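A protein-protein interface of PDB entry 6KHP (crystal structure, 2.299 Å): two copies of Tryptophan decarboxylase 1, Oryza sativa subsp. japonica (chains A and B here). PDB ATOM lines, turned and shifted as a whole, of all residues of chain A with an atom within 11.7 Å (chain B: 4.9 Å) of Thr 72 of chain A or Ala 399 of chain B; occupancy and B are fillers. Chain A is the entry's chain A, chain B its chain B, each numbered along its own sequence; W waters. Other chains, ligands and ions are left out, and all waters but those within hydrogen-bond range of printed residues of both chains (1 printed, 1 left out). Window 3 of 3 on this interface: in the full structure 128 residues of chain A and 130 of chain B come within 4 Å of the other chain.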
ATOM      1  N   THR A  21       9.798  17.538   0.709  1.00  0.00           N
ATOM      2  CA  THR A  21      10.409  17.748   2.012  1.00  0.00           C
ATOM      3  C   THR A  21      11.925  18.018   1.903  1.00  0.00           C
ATOM      4  O   THR A  21      12.483  18.717   2.746  1.00  0.00           O
ATOM      5  CB  THR A  21      10.136  16.541   2.955  1.00  0.00           C
ATOM      6  OG1 THR A  21      10.922  16.646   4.156  1.00  0.00           O
ATOM      7  CG2 THR A  21      10.419  15.211   2.253  1.00  0.00           C
ATOM      8  N   PHE A  22      12.599  17.497   0.875  1.00  0.00           N
ATOM      9  CA  PHE A  22      14.006  17.841   0.665  1.00  0.00           C
ATOM     10  C   PHE A  22      14.112  19.242   0.071  1.00  0.00           C
ATOM     11  O   PHE A  22      13.544  19.518  -0.988  1.00  0.00           O
ATOM     12  CB  PHE A  22      14.714  16.841  -0.240  1.00  0.00           C
ATOM     13  CG  PHE A  22      16.090  17.297  -0.670  1.00  0.00           C
ATOM     14  CD1 PHE A  22      17.045  17.641   0.272  1.00  0.00           C
ATOM     15  CD2 PHE A  22      16.419  17.397  -2.007  1.00  0.00           C
ATOM     16  CE1 PHE A  22      18.312  18.062  -0.117  1.00  0.00           C
ATOM     17  CE2 PHE A  22      17.677  17.819  -2.403  1.00  0.00           C
ATOM     18  CZ  PHE A  22      18.625  18.152  -1.464  1.00  0.00           C
ATOM     19  N   GLN A  23      14.857  20.116   0.747  1.00  0.00           N
ATOM     20  CA  GLN A  23      14.919  21.542   0.430  1.00  0.00           C
ATOM     21  C   GLN A  23      16.380  21.929   0.238  1.00  0.00           C
ATOM     22  O   GLN A  23      17.087  22.231   1.207  1.00  0.00           O
ATOM     23  CB  GLN A  23      14.275  22.370   1.538  1.00  0.00           C
ATOM     24  CG  GLN A  23      12.915  21.857   2.021  1.00  0.00           C
ATOM     25  CD  GLN A  23      12.254  22.773   3.061  1.00  0.00           C
ATOM     26  OE1 GLN A  23      12.929  23.461   3.842  1.00  0.00           O
ATOM     27  NE2 GLN A  23      10.922  22.782   3.066  1.00  0.00           N
ATOM     28  N   PRO A  24      16.871  21.926  -1.001  1.00  0.00           N
ATOM     29  CA  PRO A  24      18.306  22.163  -1.217  1.00  0.00           C
ATOM     30  C   PRO A  24      18.758  23.560  -0.834  1.00  0.00           C
ATOM     31  O   PRO A  24      19.953  23.758  -0.579  1.00  0.00           O
ATOM     32  CB  PRO A  24      18.483  21.910  -2.726  1.00  0.00           C
ATOM     33  CG  PRO A  24      17.152  22.202  -3.303  1.00  0.00           C
ATOM     34  CD  PRO A  24      16.137  21.754  -2.265  1.00  0.00           C
ATOM     35  N   ARG A  67      35.356   7.449  -3.659  1.00  0.00           N
ATOM     36  CA  ARG A  67      35.203   6.112  -4.229  1.00  0.00           C
ATOM     37  C   ARG A  67      34.960   6.148  -5.743  1.00  0.00           C
ATOM     38  O   ARG A  67      34.922   7.203  -6.374  1.00  0.00           O
ATOM     39  CB  ARG A  67      34.106   5.353  -3.516  1.00  0.00           C
ATOM     40  CG  ARG A  67      34.560   4.730  -2.233  1.00  0.00           C
ATOM     41  CD  ARG A  67      33.419   3.897  -1.781  1.00  0.00           C
ATOM     42  NE  ARG A  67      33.444   3.619  -0.374  1.00  0.00           N
ATOM     43  CZ  ARG A  67      32.490   2.928   0.222  1.00  0.00           C
ATOM     44  NH1 ARG A  67      31.470   2.482  -0.501  1.00  0.00           N
ATOM     45  NH2 ARG A  67      32.562   2.694   1.518  1.00  0.00           N
ATOM     46  N   ALA A  68      34.809   4.961  -6.334  1.00  0.00           N
ATOM     47  CA  ALA A  68      34.554   4.877  -7.765  1.00  0.00           C
ATOM     48  C   ALA A  68      33.122   5.263  -8.115  1.00  0.00           C
ATOM     49  O   ALA A  68      32.832   5.526  -9.290  1.00  0.00           O
ATOM     50  CB  ALA A  68      34.840   3.462  -8.275  1.00  0.00           C
ATOM     51  N   SER A  69      32.226   5.286  -7.133  1.00  0.00           N
ATOM     52  CA  SER A  69      30.805   5.461  -7.368  1.00  0.00           C
ATOM     53  C   SER A  69      30.245   6.502  -6.419  1.00  0.00           C
ATOM     54  O   SER A  69      30.766   6.673  -5.310  1.00  0.00           O
ATOM     55  CB  SER A  69      30.056   4.140  -7.178  1.00  0.00           C
ATOM     56  OG  SER A  69      30.578   3.172  -8.073  1.00  0.00           O
ATOM     57  N   PRO A  70      29.190   7.220  -6.832  1.00  0.00           N
ATOM     58  CA  PRO A  70      28.567   8.190  -5.922  1.00  0.00           C
ATOM     59  C   PRO A  70      27.844   7.481  -4.800  1.00  0.00           C
ATOM     60  O   PRO A  70      27.327   6.361  -4.984  1.00  0.00           O
ATOM     61  CB  PRO A  70      27.578   8.942  -6.833  1.00  0.00           C
ATOM     62  CG  PRO A  70      27.230   7.941  -7.914  1.00  0.00           C
ATOM     63  CD  PRO A  70      28.476   7.104  -8.120  1.00  0.00           C
ATOM     64  N   PRO A  71      27.753   8.090  -3.611  1.00  0.00           N
ATOM     65  CA  PRO A  71      27.008   7.462  -2.505  1.00  0.00           C
ATOM     66  C   PRO A  71      25.518   7.461  -2.779  1.00  0.00           C
ATOM     67  O   PRO A  71      24.979   8.373  -3.415  1.00  0.00           O
ATOM     68  CB  PRO A  71      27.333   8.346  -1.297  1.00  0.00           C
ATOM     69  CG  PRO A  71      27.624   9.723  -1.915  1.00  0.00           C
ATOM     70  CD  PRO A  71      28.309   9.408  -3.237  1.00  0.00           C
ATOM     71  N   THR A  72      24.848   6.421  -2.282  1.00  0.00           N
ATOM     72  CA  THR A  72      23.401   6.344  -2.425  1.00  0.00           C
ATOM     73  C   THR A  72      22.714   7.340  -1.496  1.00  0.00           C
ATOM     74  O   THR A  72      21.736   7.994  -1.889  1.00  0.00           O
ATOM     75  CB  THR A  72      22.929   4.910  -2.149  1.00  0.00           C
ATOM     76  OG1 THR A  72      23.572   4.032  -3.074  1.00  0.00           O
ATOM     77  CG2 THR A  72      21.440   4.781  -2.334  1.00  0.00           C
ATOM     78  N   TYR A  73      23.245   7.501  -0.287  1.00  0.00           N
ATOM     79  CA  TYR A  73      22.645   8.283   0.779  1.00  0.00           C
ATOM     80  C   TYR A  73      23.412   9.583   0.977  1.00  0.00           C
ATOM     81  O   TYR A  73      24.506   9.779   0.436  1.00  0.00           O
ATOM     82  CB  TYR A  73      22.599   7.463   2.077  1.00  0.00           C
ATOM     83  CG  TYR A  73      21.898   6.156   1.848  1.00  0.00           C
ATOM     84  CD1 TYR A  73      20.515   6.118   1.704  1.00  0.00           C
ATOM     85  CD2 TYR A  73      22.613   4.966   1.714  1.00  0.00           C
ATOM     86  CE1 TYR A  73      19.860   4.940   1.455  1.00  0.00           C
ATOM     87  CE2 TYR A  73      21.954   3.771   1.472  1.00  0.00           C
ATOM     88  CZ  TYR A  73      20.577   3.775   1.340  1.00  0.00           C
ATOM     89  OH  TYR A  73      19.893   2.614   1.092  1.00  0.00           O
ATOM     90  N   SER A  74      22.816  10.474   1.765  1.00  0.00           N
ATOM     91  CA  SER A  74      23.380  11.791   2.008  1.00  0.00           C
ATOM     92  C   SER A  74      24.400  11.742   3.138  1.00  0.00           C
ATOM     93  O   SER A  74      24.472  10.783   3.910  1.00  0.00           O
ATOM     94  CB  SER A  74      22.273  12.791   2.345  1.00  0.00           C
ATOM     95  OG  SER A  74      21.695  12.493   3.608  1.00  0.00           O
ATOM     96  N   ALA A  75      25.193  12.800   3.239  1.00  0.00           N
ATOM     97  CA  ALA A  75      26.168  12.919   4.301  1.00  0.00           C
ATOM     98  C   ALA A  75      26.186  14.359   4.783  1.00  0.00           C
ATOM     99  O   ALA A  75      25.912  15.278   4.003  1.00  0.00           O
ATOM    100  CB  ALA A  75      27.573  12.493   3.845  1.00  0.00           C
ATOM    101  N   PRO A  76      26.470  14.584   6.066  1.00  0.00           N
ATOM    102  CA  PRO A  76      26.588  15.963   6.561  1.00  0.00           C
ATOM    103  C   PRO A  76      27.637  16.719   5.769  1.00  0.00           C
ATOM    104  O   PRO A  76      28.650  16.150   5.345  1.00  0.00           O
ATOM    105  CB  PRO A  76      27.017  15.784   8.028  1.00  0.00           C
ATOM    106  CG  PRO A  76      26.583  14.391   8.388  1.00  0.00           C
ATOM    107  CD  PRO A  76      26.710  13.586   7.124  1.00  0.00           C
ATOM    108  N   GLU A  83      36.497  15.694   3.322  1.00  0.00           N
ATOM    109  CA  GLU A  83      37.110  15.104   2.139  1.00  0.00           C
ATOM    110  C   GLU A  83      37.767  16.170   1.262  1.00  0.00           C
ATOM    111  O   GLU A  83      38.797  15.907   0.635  1.00  0.00           O
ATOM    112  CB  GLU A  83      36.064  14.296   1.371  1.00  0.00           C
ATOM    113  CG  GLU A  83      35.628  13.059   2.146  1.00  0.00           C
ATOM    114  CD  GLU A  83      34.546  12.260   1.456  1.00  0.00           C
ATOM    115  OE1 GLU A  83      34.084  12.692   0.385  1.00  0.00           O
ATOM    116  OE2 GLU A  83      34.150  11.197   1.988  1.00  0.00           O
ATOM    117  N   TYR B 396      24.503  15.028  -1.042  1.00  0.00           N
ATOM    118  CA  TYR B 396      23.096  14.624  -1.090  1.00  0.00           C
ATOM    119  C   TYR B 396      22.886  13.166  -1.473  1.00  0.00           C
ATOM    120  O   TYR B 396      21.893  12.571  -1.051  1.00  0.00           O
ATOM    121  CB  TYR B 396      22.311  15.521  -2.058  1.00  0.00           C
ATOM    122  CG  TYR B 396      22.438  17.002  -1.734  1.00  0.00           C
ATOM    123  CD1 TYR B 396      22.201  17.474  -0.446  1.00  0.00           C
ATOM    124  CD2 TYR B 396      22.803  17.923  -2.717  1.00  0.00           C
ATOM    125  CE1 TYR B 396      22.321  18.822  -0.140  1.00  0.00           C
ATOM    126  CE2 TYR B 396      22.924  19.272  -2.430  1.00  0.00           C
ATOM    127  CZ  TYR B 396      22.688  19.717  -1.137  1.00  0.00           C
ATOM    128  OH  TYR B 396      22.812  21.056  -0.847  1.00  0.00           O
ATOM    129  N   GLY B 397      23.775  12.574  -2.258  1.00  0.00           N
ATOM    130  CA  GLY B 397      23.637  11.187  -2.642  1.00  0.00           C
ATOM    131  C   GLY B 397      22.641  10.980  -3.772  1.00  0.00           C
ATOM    132  O   GLY B 397      21.795  11.822  -4.068  1.00  0.00           O
ATOM    133  N   VAL B 398      22.737   9.804  -4.397  1.00  0.00           N
ATOM    134  CA  VAL B 398      21.932   9.528  -5.581  1.00  0.00           C
ATOM    135  C   VAL B 398      20.454   9.569  -5.248  1.00  0.00           C
ATOM    136  O   VAL B 398      19.649  10.106  -6.016  1.00  0.00           O
ATOM    137  CB  VAL B 398      22.322   8.176  -6.205  1.00  0.00           C
ATOM    138  CG1 VAL B 398      21.411   7.857  -7.386  1.00  0.00           C
ATOM    139  CG2 VAL B 398      23.786   8.197  -6.653  1.00  0.00           C
ATOM    140  N   ALA B 399      20.063   8.991  -4.110  1.00  0.00           N
ATOM    141  CA  ALA B 399      18.636   8.850  -3.842  1.00  0.00           C
ATOM    142  C   ALA B 399      17.957  10.212  -3.724  1.00  0.00           C
ATOM    143  O   ALA B 399      16.848  10.403  -4.232  1.00  0.00           O
ATOM    144  CB  ALA B 399      18.406   8.015  -2.581  1.00  0.00           C
ATOM    145  N   LYS B 400      18.604  11.176  -3.062  1.00  0.00           N
ATOM    146  CA  LYS B 400      17.989  12.495  -2.962  1.00  0.00           C
ATOM    147  C   LYS B 400      17.979  13.198  -4.309  1.00  0.00           C
ATOM    148  O   LYS B 400      17.023  13.915  -4.622  1.00  0.00           O
ATOM    149  CB  LYS B 400      18.702  13.341  -1.910  1.00  0.00           C
ATOM    150  CG  LYS B 400      18.307  12.937  -0.505  1.00  0.00           C
ATOM    151  CD  LYS B 400      18.824  13.874   0.562  1.00  0.00           C
ATOM    152  CE  LYS B 400      18.310  13.406   1.918  1.00  0.00           C
ATOM    153  NZ  LYS B 400      18.963  14.144   3.017  1.00  0.00           N
ATOM    154  N   LEU B 401      19.006  12.977  -5.132  1.00  0.00           N
ATOM    155  CA  LEU B 401      18.994  13.561  -6.466  1.00  0.00           C
ATOM    156  C   LEU B 401      17.817  13.020  -7.266  1.00  0.00           C
ATOM    157  O   LEU B 401      17.115  13.783  -7.941  1.00  0.00           O
ATOM    158  CB  LEU B 401      20.325  13.306  -7.178  1.00  0.00           C
ATOM    159  CG  LEU B 401      21.549  14.000  -6.571  1.00  0.00           C
ATOM    160  CD1 LEU B 401      22.766  13.849  -7.458  1.00  0.00           C
ATOM    161  CD2 LEU B 401      21.287  15.470  -6.340  1.00  0.00           C
ATOM    162  N   GLN B 402      17.542  11.717  -7.139  1.00  0.00           N
ATOM    163  CA  GLN B 402      16.418  11.118  -7.852  1.00  0.00           C
ATOM    164  C   GLN B 402      15.081  11.632  -7.334  1.00  0.00           C
ATOM    165  O   GLN B 402      14.162  11.892  -8.120  1.00  0.00           O
ATOM    166  CB  GLN B 402      16.470   9.595  -7.736  1.00  0.00           C
ATOM    167  CG  GLN B 402      17.706   8.959  -8.346  1.00  0.00           C
ATOM    168  CD  GLN B 402      17.713   7.463  -8.143  1.00  0.00           C
ATOM    169  OE1 GLN B 402      17.572   6.984  -7.020  1.00  0.00           O
ATOM    170  NE2 GLN B 402      17.853   6.714  -9.227  1.00  0.00           N
ATOM    171  N   GLU B 403      14.929  11.753  -6.018  1.00  0.00           N
ATOM    172  CA  GLU B 403      13.660  12.258  -5.502  1.00  0.00           C
ATOM    173  C   GLU B 403      13.467  13.732  -5.849  1.00  0.00           C
ATOM    174  O   GLU B 403      12.326  14.190  -5.976  1.00  0.00           O
ATOM    175  CB  GLU B 403      13.564  12.027  -3.989  1.00  0.00           C
ATOM    176  CG  GLU B 403      12.227  12.462  -3.366  1.00  0.00           C
ATOM    177  CD  GLU B 403      10.975  11.829  -4.020  1.00  0.00           C
ATOM    178  OE1 GLU B 403       9.940  12.535  -4.152  1.00  0.00           O
ATOM    179  OE2 GLU B 403      11.008  10.624  -4.386  1.00  0.00           O
HETATM  180  O   HOH W   1      21.518  22.133   1.026  1.00  0.00           O
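No position is printed for both chains.
Of the 15 printed residues of chain A, 7 touch a printed residue of chain B. Hydrophobic or aromatic side chains of chain B within 4 Å of the printed part of chain A: Tyr 396, Val 398 and Ala 399. Among the printed residues, 12 pairs touch across the chains. Among the printed residues, no Asp or Glu carboxylate lies within 4 Å of a Lys or Arg side-chain nitrogen of the other chain.
Thr 21 of chain A touches none of the printed residues of chain B. Of the printed residues of chain B, Phe 22 of chain A touches Tyr 396. Of the printed residues of chain B, Pro 71 of chain A touches Gly 397 (3.2 Å) and Val 398 (2.8 Å). Thr 72 of chain A touches three residues of chain B. Of the printed residues of chain B, Tyr 73 of chain A touches Tyr 396 and Gly 397. Of the printed residues of chain B, Ser 74 of chain A touches Tyr 396 (3.4 Å) and Lys 400 (3.2 Å). No residue of chain A comes within 4 Å of Leu 401 of chain B. No residue of chain A comes within 4 Å of Gln 402 of chain B. The nearest printed residue of chain A that does not touch Tyr 396 of chain B is Thr 72 of chain A (4.7 Å).
The backbone NH of Val 398 of chain B lies within hydrogen-bond range of the backbone carbonyl oxygen of Pro 71 of chain A. N of Val 398 of chain B sits at hydrogen-bond distance from O of Thr 72 of chain A, 3.3 Å away. The backbone carbonyl oxygen (O) of Thr 72 of chain A sits at hydrogen-bond distance from the backbone NH (N) of Ala 399 of chain B (3.0 Å). The side-chain hydroxyl (OG) of Ser 74 of chain A is in hydrogen-bond range of the side-chain amino group (NZ) of Lys 400 of chain B, 3.2 Å away.
Water W1 bridges the side-chain hydroxyl (OH) of Tyr 396 of chain B (2.5 Å) and the backbone carbonyl oxygen (O) of Pro 24 of chain A (2.8 Å).
Among the printed residues, pairs that only touch across the chains: Phe 22 of chain A with Tyr 396 of chain B, Pro 24 of chain A with Tyr 396 of chain B, Pro 70 of chain A with Val 398 of chain B, Pro 71 of chain A with Gly 397 of chain B, Thr 72 of chain A with Gly 397 of chain B, Tyr 73 of chain A with Tyr 396 of chain B, Tyr 73 of chain A with Gly 397 of chain B and Ser 74 of chain A with Tyr 396 of chain B.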
